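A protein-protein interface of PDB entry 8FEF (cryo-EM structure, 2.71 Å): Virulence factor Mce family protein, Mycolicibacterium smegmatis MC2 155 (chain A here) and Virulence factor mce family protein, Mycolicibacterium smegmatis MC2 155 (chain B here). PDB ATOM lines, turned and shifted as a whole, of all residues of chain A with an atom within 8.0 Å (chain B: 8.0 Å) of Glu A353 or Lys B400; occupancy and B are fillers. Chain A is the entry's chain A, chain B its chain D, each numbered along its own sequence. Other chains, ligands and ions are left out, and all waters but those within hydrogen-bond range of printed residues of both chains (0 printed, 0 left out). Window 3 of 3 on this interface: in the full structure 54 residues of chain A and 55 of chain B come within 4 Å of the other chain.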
ATOM      1  N   GLY A 350       8.501  28.015  -0.640  1.00  0.00           N
ATOM      2  CA  GLY A 350       7.318  27.175  -0.715  1.00  0.00           C
ATOM      3  C   GLY A 350       7.389  25.923   0.146  1.00  0.00           C
ATOM      4  O   GLY A 350       8.122  25.836   1.130  1.00  0.00           O
ATOM      5  N   GLY A 351       6.582  24.940  -0.243  1.00  0.00           N
ATOM      6  CA  GLY A 351       6.522  23.671   0.442  1.00  0.00           C
ATOM      7  C   GLY A 351       5.772  22.646  -0.382  1.00  0.00           C
ATOM      8  O   GLY A 351       5.587  22.818  -1.590  1.00  0.00           O
ATOM      9  N   PRO A 352       5.347  21.549   0.245  1.00  0.00           N
ATOM     10  CA  PRO A 352       4.572  20.537  -0.484  1.00  0.00           C
ATOM     11  C   PRO A 352       3.290  21.113  -1.068  1.00  0.00           C
ATOM     12  O   PRO A 352       2.585  21.886  -0.418  1.00  0.00           O
ATOM     13  CB  PRO A 352       4.278  19.477   0.583  1.00  0.00           C
ATOM     14  CG  PRO A 352       4.542  20.138   1.884  1.00  0.00           C
ATOM     15  CD  PRO A 352       5.622  21.132   1.627  1.00  0.00           C
ATOM     16  N   GLU A 353       3.003  20.725  -2.312  1.00  0.00           N
ATOM     17  CA  GLU A 353       1.809  21.153  -3.047  1.00  0.00           C
ATOM     18  C   GLU A 353       1.778  22.664  -3.267  1.00  0.00           C
ATOM     19  O   GLU A 353       0.709  23.255  -3.438  1.00  0.00           O
ATOM     20  CB  GLU A 353       0.526  20.680  -2.360  1.00  0.00           C
ATOM     21  CG  GLU A 353       0.414  19.172  -2.273  1.00  0.00           C
ATOM     22  CD  GLU A 353       0.489  18.506  -3.632  1.00  0.00           C
ATOM     23  OE1 GLU A 353      -0.120  19.030  -4.589  1.00  0.00           O
ATOM     24  OE2 GLU A 353       1.161  17.460  -3.746  1.00  0.00           O
ATOM     25  N   GLY A 354       2.948  23.301  -3.274  1.00  0.00           N
ATOM     26  CA  GLY A 354       3.057  24.710  -3.575  1.00  0.00           C
ATOM     27  C   GLY A 354       2.959  25.643  -2.388  1.00  0.00           C
ATOM     28  O   GLY A 354       3.246  26.836  -2.538  1.00  0.00           O
ATOM     29  N   ARG A 355       2.573  25.145  -1.219  1.00  0.00           N
ATOM     30  CA  ARG A 355       2.405  25.951  -0.022  1.00  0.00           C
ATOM     31  C   ARG A 355       3.160  25.308   1.130  1.00  0.00           C
ATOM     32  O   ARG A 355       3.370  24.092   1.128  1.00  0.00           O
ATOM     33  CB  ARG A 355       0.918  26.094   0.339  1.00  0.00           C
ATOM     34  CG  ARG A 355       0.076  26.660  -0.787  1.00  0.00           C
ATOM     35  CD  ARG A 355      -1.314  27.077  -0.332  1.00  0.00           C
ATOM     36  NE  ARG A 355      -2.211  25.949  -0.117  1.00  0.00           N
ATOM     37  CZ  ARG A 355      -2.707  25.600   1.061  1.00  0.00           C
ATOM     38  NH1 ARG A 355      -2.408  26.269   2.162  1.00  0.00           N
ATOM     39  NH2 ARG A 355      -3.532  24.560   1.136  1.00  0.00           N
ATOM     40  N   PRO A 356       3.602  26.095   2.114  1.00  0.00           N
ATOM     41  CA  PRO A 356       4.345  25.511   3.239  1.00  0.00           C
ATOM     42  C   PRO A 356       3.498  24.517   4.021  1.00  0.00           C
ATOM     43  O   PRO A 356       2.296  24.709   4.210  1.00  0.00           O
ATOM     44  CB  PRO A 356       4.720  26.729   4.089  1.00  0.00           C
ATOM     45  CG  PRO A 356       3.765  27.790   3.686  1.00  0.00           C
ATOM     46  CD  PRO A 356       3.488  27.557   2.238  1.00  0.00           C
ATOM     47  N   GLY A 357       4.142  23.450   4.475  1.00  0.00           N
ATOM     48  CA  GLY A 357       3.448  22.406   5.198  1.00  0.00           C
ATOM     49  C   GLY A 357       4.355  21.206   5.380  1.00  0.00           C
ATOM     50  O   GLY A 357       5.569  21.287   5.180  1.00  0.00           O
ATOM     51  N   CYS A 358       3.741  20.093   5.769  1.00  0.00           N
ATOM     52  CA  CYS A 358       4.438  18.821   5.886  1.00  0.00           C
ATOM     53  C   CYS A 358       3.613  17.734   5.216  1.00  0.00           C
ATOM     54  O   CYS A 358       2.390  17.842   5.103  1.00  0.00           O
ATOM     55  CB  CYS A 358       4.686  18.416   7.346  1.00  0.00           C
ATOM     56  SG  CYS A 358       5.519  19.606   8.409  1.00  0.00           S
ATOM     57  N   TRP A 359       4.294  16.685   4.770  1.00  0.00           N
ATOM     58  CA  TRP A 359       3.592  15.496   4.313  1.00  0.00           C
ATOM     59  C   TRP A 359       2.970  14.780   5.503  1.00  0.00           C
ATOM     60  O   TRP A 359       3.444  14.891   6.636  1.00  0.00           O
ATOM     61  CB  TRP A 359       4.542  14.549   3.579  1.00  0.00           C
ATOM     62  CG  TRP A 359       5.242  15.155   2.404  1.00  0.00           C
ATOM     63  CD1 TRP A 359       6.567  15.459   2.310  1.00  0.00           C
ATOM     64  CD2 TRP A 359       4.655  15.527   1.153  1.00  0.00           C
ATOM     65  NE1 TRP A 359       6.842  15.999   1.079  1.00  0.00           N
ATOM     66  CE2 TRP A 359       5.683  16.051   0.350  1.00  0.00           C
ATOM     67  CE3 TRP A 359       3.360  15.467   0.635  1.00  0.00           C
ATOM     68  CZ2 TRP A 359       5.457  16.512  -0.942  1.00  0.00           C
ATOM     69  CZ3 TRP A 359       3.137  15.929  -0.645  1.00  0.00           C
ATOM     70  CH2 TRP A 359       4.180  16.443  -1.419  1.00  0.00           C
ATOM     71  N   PRO A 370       7.386  11.936  -1.260  1.00  0.00           N
ATOM     72  CA  PRO A 370       7.383  12.646  -2.544  1.00  0.00           C
ATOM     73  C   PRO A 370       8.546  13.622  -2.595  1.00  0.00           C
ATOM     74  O   PRO A 370       8.658  14.521  -1.760  1.00  0.00           O
ATOM     75  CB  PRO A 370       6.029  13.363  -2.552  1.00  0.00           C
ATOM     76  CG  PRO A 370       5.201  12.631  -1.564  1.00  0.00           C
ATOM     77  CD  PRO A 370       6.148  12.168  -0.503  1.00  0.00           C
ATOM     78  N   LEU A 372      10.642  16.689  -3.284  1.00  0.00           N
ATOM     79  CA  LEU A 372      10.242  18.084  -3.404  1.00  0.00           C
ATOM     80  C   LEU A 372      11.302  18.843  -4.187  1.00  0.00           C
ATOM     81  O   LEU A 372      12.480  18.843  -3.812  1.00  0.00           O
ATOM     82  CB  LEU A 372      10.033  18.714  -2.029  1.00  0.00           C
ATOM     83  CG  LEU A 372       9.270  20.036  -2.001  1.00  0.00           C
ATOM     84  CD1 LEU A 372       7.812  19.819  -2.351  1.00  0.00           C
ATOM     85  CD2 LEU A 372       9.405  20.693  -0.644  1.00  0.00           C
ATOM     86  N   VAL A 373      10.877  19.493  -5.265  1.00  0.00           N
ATOM     87  CA  VAL A 373      11.761  20.210  -6.175  1.00  0.00           C
ATOM     88  C   VAL A 373      11.675  21.695  -5.857  1.00  0.00           C
ATOM     89  O   VAL A 373      10.582  22.274  -5.847  1.00  0.00           O
ATOM     90  CB  VAL A 373      11.390  19.934  -7.641  1.00  0.00           C
ATOM     91  CG1 VAL A 373      12.265  20.747  -8.574  1.00  0.00           C
ATOM     92  CG2 VAL A 373      11.516  18.453  -7.945  1.00  0.00           C
ATOM     93  N   GLN B 394       6.007  10.396  -8.338  1.00  0.00           N
ATOM     94  CA  GLN B 394       6.454  10.788  -7.010  1.00  0.00           C
ATOM     95  C   GLN B 394       6.888  12.242  -6.913  1.00  0.00           C
ATOM     96  O   GLN B 394       6.961  12.773  -5.801  1.00  0.00           O
ATOM     97  CB  GLN B 394       7.619   9.900  -6.561  1.00  0.00           C
ATOM     98  CG  GLN B 394       7.297   8.424  -6.536  1.00  0.00           C
ATOM     99  CD  GLN B 394       8.469   7.596  -6.071  1.00  0.00           C
ATOM    100  OE1 GLN B 394       9.516   8.133  -5.717  1.00  0.00           O
ATOM    101  NE2 GLN B 394       8.303   6.280  -6.070  1.00  0.00           N
ATOM    102  N   ILE B 395       7.181  12.895  -8.036  1.00  0.00           N
ATOM    103  CA  ILE B 395       7.778  14.224  -7.995  1.00  0.00           C
ATOM    104  C   ILE B 395       6.735  15.248  -7.571  1.00  0.00           C
ATOM    105  O   ILE B 395       5.629  15.301  -8.122  1.00  0.00           O
ATOM    106  CB  ILE B 395       8.388  14.584  -9.355  1.00  0.00           C
ATOM    107  CG1 ILE B 395       9.348  13.490  -9.814  1.00  0.00           C
ATOM    108  CG2 ILE B 395       9.125  15.901  -9.270  1.00  0.00           C
ATOM    109  CD1 ILE B 395      10.485  13.247  -8.855  1.00  0.00           C
ATOM    110  N   ALA B 396       7.087  16.063  -6.582  1.00  0.00           N
ATOM    111  CA  ALA B 396       6.287  17.198  -6.156  1.00  0.00           C
ATOM    112  C   ALA B 396       7.152  18.447  -6.209  1.00  0.00           C
ATOM    113  O   ALA B 396       8.371  18.381  -6.030  1.00  0.00           O
ATOM    114  CB  ALA B 396       5.730  16.999  -4.746  1.00  0.00           C
ATOM    115  N   TYR B 397       6.522  19.586  -6.474  1.00  0.00           N
ATOM    116  CA  TYR B 397       7.236  20.836  -6.691  1.00  0.00           C
ATOM    117  C   TYR B 397       6.943  21.805  -5.558  1.00  0.00           C
ATOM    118  O   TYR B 397       5.786  21.973  -5.162  1.00  0.00           O
ATOM    119  CB  TYR B 397       6.856  21.446  -8.040  1.00  0.00           C
ATOM    120  CG  TYR B 397       7.198  20.547  -9.203  1.00  0.00           C
ATOM    121  CD1 TYR B 397       8.501  20.441  -9.662  1.00  0.00           C
ATOM    122  CD2 TYR B 397       6.219  19.792  -9.831  1.00  0.00           C
ATOM    123  CE1 TYR B 397       8.820  19.613 -10.715  1.00  0.00           C
ATOM    124  CE2 TYR B 397       6.529  18.962 -10.887  1.00  0.00           C
ATOM    125  CZ  TYR B 397       7.830  18.877 -11.325  1.00  0.00           C
ATOM    126  OH  TYR B 397       8.142  18.052 -12.378  1.00  0.00           O
ATOM    127  N   SER B 398       8.000  22.433  -5.037  1.00  0.00           N
ATOM    128  CA  SER B 398       7.843  23.377  -3.938  1.00  0.00           C
ATOM    129  C   SER B 398       7.030  24.590  -4.367  1.00  0.00           C
ATOM    130  O   SER B 398       6.228  25.118  -3.590  1.00  0.00           O
ATOM    131  CB  SER B 398       9.213  23.805  -3.419  1.00  0.00           C
ATOM    132  OG  SER B 398       9.083  24.616  -2.272  1.00  0.00           O
ATOM    133  N   GLU B 399       7.235  25.051  -5.594  1.00  0.00           N
ATOM    134  CA  GLU B 399       6.497  26.165  -6.163  1.00  0.00           C
ATOM    135  C   GLU B 399       5.805  25.700  -7.434  1.00  0.00           C
ATOM    136  O   GLU B 399       6.330  24.864  -8.173  1.00  0.00           O
ATOM    137  CB  GLU B 399       7.419  27.343  -6.478  1.00  0.00           C
ATOM    138  CG  GLU B 399       8.020  28.008  -5.261  1.00  0.00           C
ATOM    139  CD  GLU B 399       9.322  28.708  -5.575  1.00  0.00           C
ATOM    140  OE1 GLU B 399      10.310  28.012  -5.884  1.00  0.00           O
ATOM    141  OE2 GLU B 399       9.355  29.954  -5.520  1.00  0.00           O
ATOM    142  N   LYS B 400       4.622  26.250  -7.690  1.00  0.00           N
ATOM    143  CA  LYS B 400       3.880  25.865  -8.880  1.00  0.00           C
ATOM    144  C   LYS B 400       4.413  26.509 -10.151  1.00  0.00           C
ATOM    145  O   LYS B 400       3.932  26.181 -11.239  1.00  0.00           O
ATOM    146  CB  LYS B 400       2.398  26.198  -8.700  1.00  0.00           C
ATOM    147  CG  LYS B 400       1.670  25.194  -7.820  1.00  0.00           C
ATOM    148  CD  LYS B 400       0.210  25.555  -7.629  1.00  0.00           C
ATOM    149  CE  LYS B 400      -0.555  24.398  -7.007  1.00  0.00           C
ATOM    150  NZ  LYS B 400       0.083  23.921  -5.749  1.00  0.00           N
ATOM    151  N   ARG B 401       5.385  27.415 -10.044  1.00  0.00           N
ATOM    152  CA  ARG B 401       6.056  27.952 -11.218  1.00  0.00           C
ATOM    153  C   ARG B 401       7.171  27.048 -11.726  1.00  0.00           C
ATOM    154  O   ARG B 401       7.656  27.260 -12.841  1.00  0.00           O
ATOM    155  CB  ARG B 401       6.633  29.334 -10.918  1.00  0.00           C
ATOM    156  CG  ARG B 401       7.852  29.299 -10.027  1.00  0.00           C
ATOM    157  CD  ARG B 401       8.496  30.658  -9.933  1.00  0.00           C
ATOM    158  NE  ARG B 401       9.737  30.609  -9.174  1.00  0.00           N
ATOM    159  CZ  ARG B 401      10.908  30.261  -9.685  1.00  0.00           C
ATOM    160  NH1 ARG B 401      11.033  29.925 -10.957  1.00  0.00           N
ATOM    161  NH2 ARG B 401      11.981  30.258  -8.903  1.00  0.00           N
ATOM    162  N   LEU B 402       7.591  26.061 -10.938  1.00  0.00           N
ATOM    163  CA  LEU B 402       8.643  25.139 -11.335  1.00  0.00           C
ATOM    164  C   LEU B 402       8.118  23.903 -12.051  1.00  0.00           C
ATOM    165  O   LEU B 402       8.921  23.128 -12.582  1.00  0.00           O
ATOM    166  CB  LEU B 402       9.449  24.703 -10.107  1.00  0.00           C
ATOM    167  CG  LEU B 402      10.359  25.742  -9.454  1.00  0.00           C
ATOM    168  CD1 LEU B 402      10.687  25.341  -8.033  1.00  0.00           C
ATOM    169  CD2 LEU B 402      11.629  25.895 -10.261  1.00  0.00           C
ATOM    170  N   GLN B 403       6.808  23.703 -12.087  1.00  0.00           N
ATOM    171  CA  GLN B 403       6.243  22.499 -12.684  1.00  0.00           C
ATOM    172  C   GLN B 403       6.222  22.627 -14.202  1.00  0.00           C
ATOM    173  O   GLN B 403       5.674  23.601 -14.727  1.00  0.00           O
ATOM    174  CB  GLN B 403       4.834  22.256 -12.161  1.00  0.00           C
ATOM    175  CG  GLN B 403       4.174  21.017 -12.729  1.00  0.00           C
ATOM    176  CD  GLN B 403       2.715  20.914 -12.349  1.00  0.00           C
ATOM    177  OE1 GLN B 403       2.164  21.809 -11.710  1.00  0.00           O
ATOM    178  NE2 GLN B 403       2.079  19.817 -12.738  1.00  0.00           N
ATOM    179  N   PRO B 404       6.810  21.679 -14.935  1.00  0.00           N
ATOM    180  CA  PRO B 404       6.852  21.801 -16.389  1.00  0.00           C
ATOM    181  C   PRO B 404       5.464  21.701 -16.990  1.00  0.00           C
ATOM    182  O   PRO B 404       4.589  20.995 -16.458  1.00  0.00           O
ATOM    183  CB  PRO B 404       7.734  20.614 -16.818  1.00  0.00           C
ATOM    184  CG  PRO B 404       8.499  20.243 -15.598  1.00  0.00           C
ATOM    185  CD  PRO B 404       7.580  20.520 -14.457  1.00  0.00           C
ATOM    186  N   PRO B 405       5.212  22.386 -18.101  1.00  0.00           N
ATOM    187  CA  PRO B 405       3.941  22.236 -18.805  1.00  0.00           C
ATOM    188  C   PRO B 405       3.960  20.982 -19.661  1.00  0.00           C
ATOM    189  O   PRO B 405       4.993  20.296 -19.721  1.00  0.00           O
ATOM    190  CB  PRO B 405       3.875  23.509 -19.662  1.00  0.00           C
ATOM    191  CG  PRO B 405       5.289  23.817 -19.949  1.00  0.00           C
ATOM    192  CD  PRO B 405       6.082  23.382 -18.746  1.00  0.00           C
ATOM    193  N   TRP B 417      13.573  23.314 -18.219  1.00  0.00           N
ATOM    194  CA  TRP B 417      12.686  22.265 -18.704  1.00  0.00           C
ATOM    195  C   TRP B 417      13.126  21.809 -20.088  1.00  0.00           C
ATOM    196  O   TRP B 417      13.149  22.608 -21.028  1.00  0.00           O
ATOM    197  CB  TRP B 417      11.245  22.767 -18.752  1.00  0.00           C
ATOM    198  CG  TRP B 417      10.751  23.293 -17.448  1.00  0.00           C
ATOM    199  CD1 TRP B 417      11.144  22.904 -16.204  1.00  0.00           C
ATOM    200  CD2 TRP B 417       9.777  24.323 -17.257  1.00  0.00           C
ATOM    201  NE1 TRP B 417      10.467  23.620 -15.248  1.00  0.00           N
ATOM    202  CE2 TRP B 417       9.623  24.500 -15.871  1.00  0.00           C
ATOM    203  CE3 TRP B 417       9.018  25.111 -18.125  1.00  0.00           C
ATOM    204  CZ2 TRP B 417       8.740  25.430 -15.334  1.00  0.00           C
ATOM    205  CZ3 TRP B 417       8.144  26.032 -17.590  1.00  0.00           C
ATOM    206  CH2 TRP B 417       8.011  26.185 -16.208  1.00  0.00           C
ATOM    207  N   ALA B 435      11.921  28.167 -16.403  1.00  0.00           N
ATOM    208  CA  ALA B 435      10.880  28.681 -15.530  1.00  0.00           C
ATOM    209  C   ALA B 435      11.054  30.184 -15.318  1.00  0.00           C
ATOM    210  O   ALA B 435      12.167  30.707 -15.415  1.00  0.00           O
ATOM    211  CB  ALA B 435      10.918  27.965 -14.184  1.00  0.00           C
ATOM    212  N   PRO B 436       9.965  30.905 -15.048  1.00  0.00           N
ATOM    213  CA  PRO B 436      10.091  32.334 -14.745  1.00  0.00           C
ATOM    214  C   PRO B 436      10.897  32.572 -13.479  1.00  0.00           C
ATOM    215  O   PRO B 436      10.873  31.775 -12.539  1.00  0.00           O
ATOM    216  CB  PRO B 436       8.637  32.790 -14.577  1.00  0.00           C
ATOM    217  CG  PRO B 436       7.839  31.796 -15.344  1.00  0.00           C
ATOM    218  CD  PRO B 436       8.557  30.493 -15.178  1.00  0.00           C
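OG of Ser B398 touches C of Gly A350, at 3.2 Å.
Gly A351 touches Tyr B397 (O to O, 3.7 Å).
CA of Gly A354 touches O of Ser B398, 3.2 Å away.
Lys B400 touches Gly A354.
CB of Ala B396 touches CH2 of Trp A359 (3.7 Å).
CA of Leu A372 touches O of Ala B396 (3.2 Å).
CD1 of Leu A372 touches C of Tyr B397, at 3.9 Å.
Leu A372 touches Ser B398.
Tyr B397 touches Val A373.
CD1 of Leu B402 touches O of Val A373 (3.8 Å).
The backbone carbonyl oxygen (O) of Leu B402 sits at hydrogen-bond distance from the indole nitrogen (NE1) of Trp B417 (3.1 Å).
The backbone NH (N) of Gly A351 lies within hydrogen-bond range of the side-chain hydroxyl (OG) of Ser B398.
The side-chain amino group of Lys B400 lies within hydrogen-bond range of the backbone carbonyl oxygen of Glu A353 (2.5 Å).
The backbone NH (N) of Val A373 sits at hydrogen-bond distance from the backbone carbonyl oxygen (O) of Ala B396 (2.8 Å).
O of Val A373 sits at hydrogen-bond distance from N of Ser B398, at 2.7 Å.
Glu A353 touches just one residue of chain B: Lys B400.
Of the printed residues of chain A, Tyr B397 touches Gly A351 (3.7 Å), Gly A354 (3.7 Å), Leu A372 (3.9 Å) and Val A373 (3.6 Å).
Of the printed residues of chain B, Val A373 touches Ile B395, Ala B396, Tyr B397, Ser B398 and Leu B402.
Of the printed residues of chain A, Ala B396 touches Trp A359 (3.7 Å), Leu A372 (3.2 Å) and Val A373 (2.8 Å).
Of the printed residues of chain B, Gly A351 touches Tyr B397 (3.7 Å) and Ser B398 (3.1 Å).
Pro B436 touches none of the printed residues of chain A.
Arg A355 touches none of the printed residues of chain B.
The nearest residue of chain B that does not touch Glu A353 is Tyr B397 (4.2 Å).
The nearest printed residue of chain A that does not touch Tyr B397 is Glu A353 (4.2 Å).
Hydrophobic or aromatic side chains of chain A that line the printed part of chain B: Trp A359, Pro A370, Leu A372 and Val A373.
Printed residues of chain B that touch a printed residue of chain A: Gln B394, Ile B395, Ala B396, Tyr B397, Ser B398, Lys B400 and Leu B402.
Hydrophobic or aromatic side chains of chain B within 4 Å of the printed part of chain A: Ile B395, Ala B396, Tyr B397 and Leu B402.
Among the printed residues, 17 pairs touch across the chains.
Among the printed residues, no Asp or Glu carboxylate lies within 4 Å of a Lys or Arg side-chain nitrogen of the other chain.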
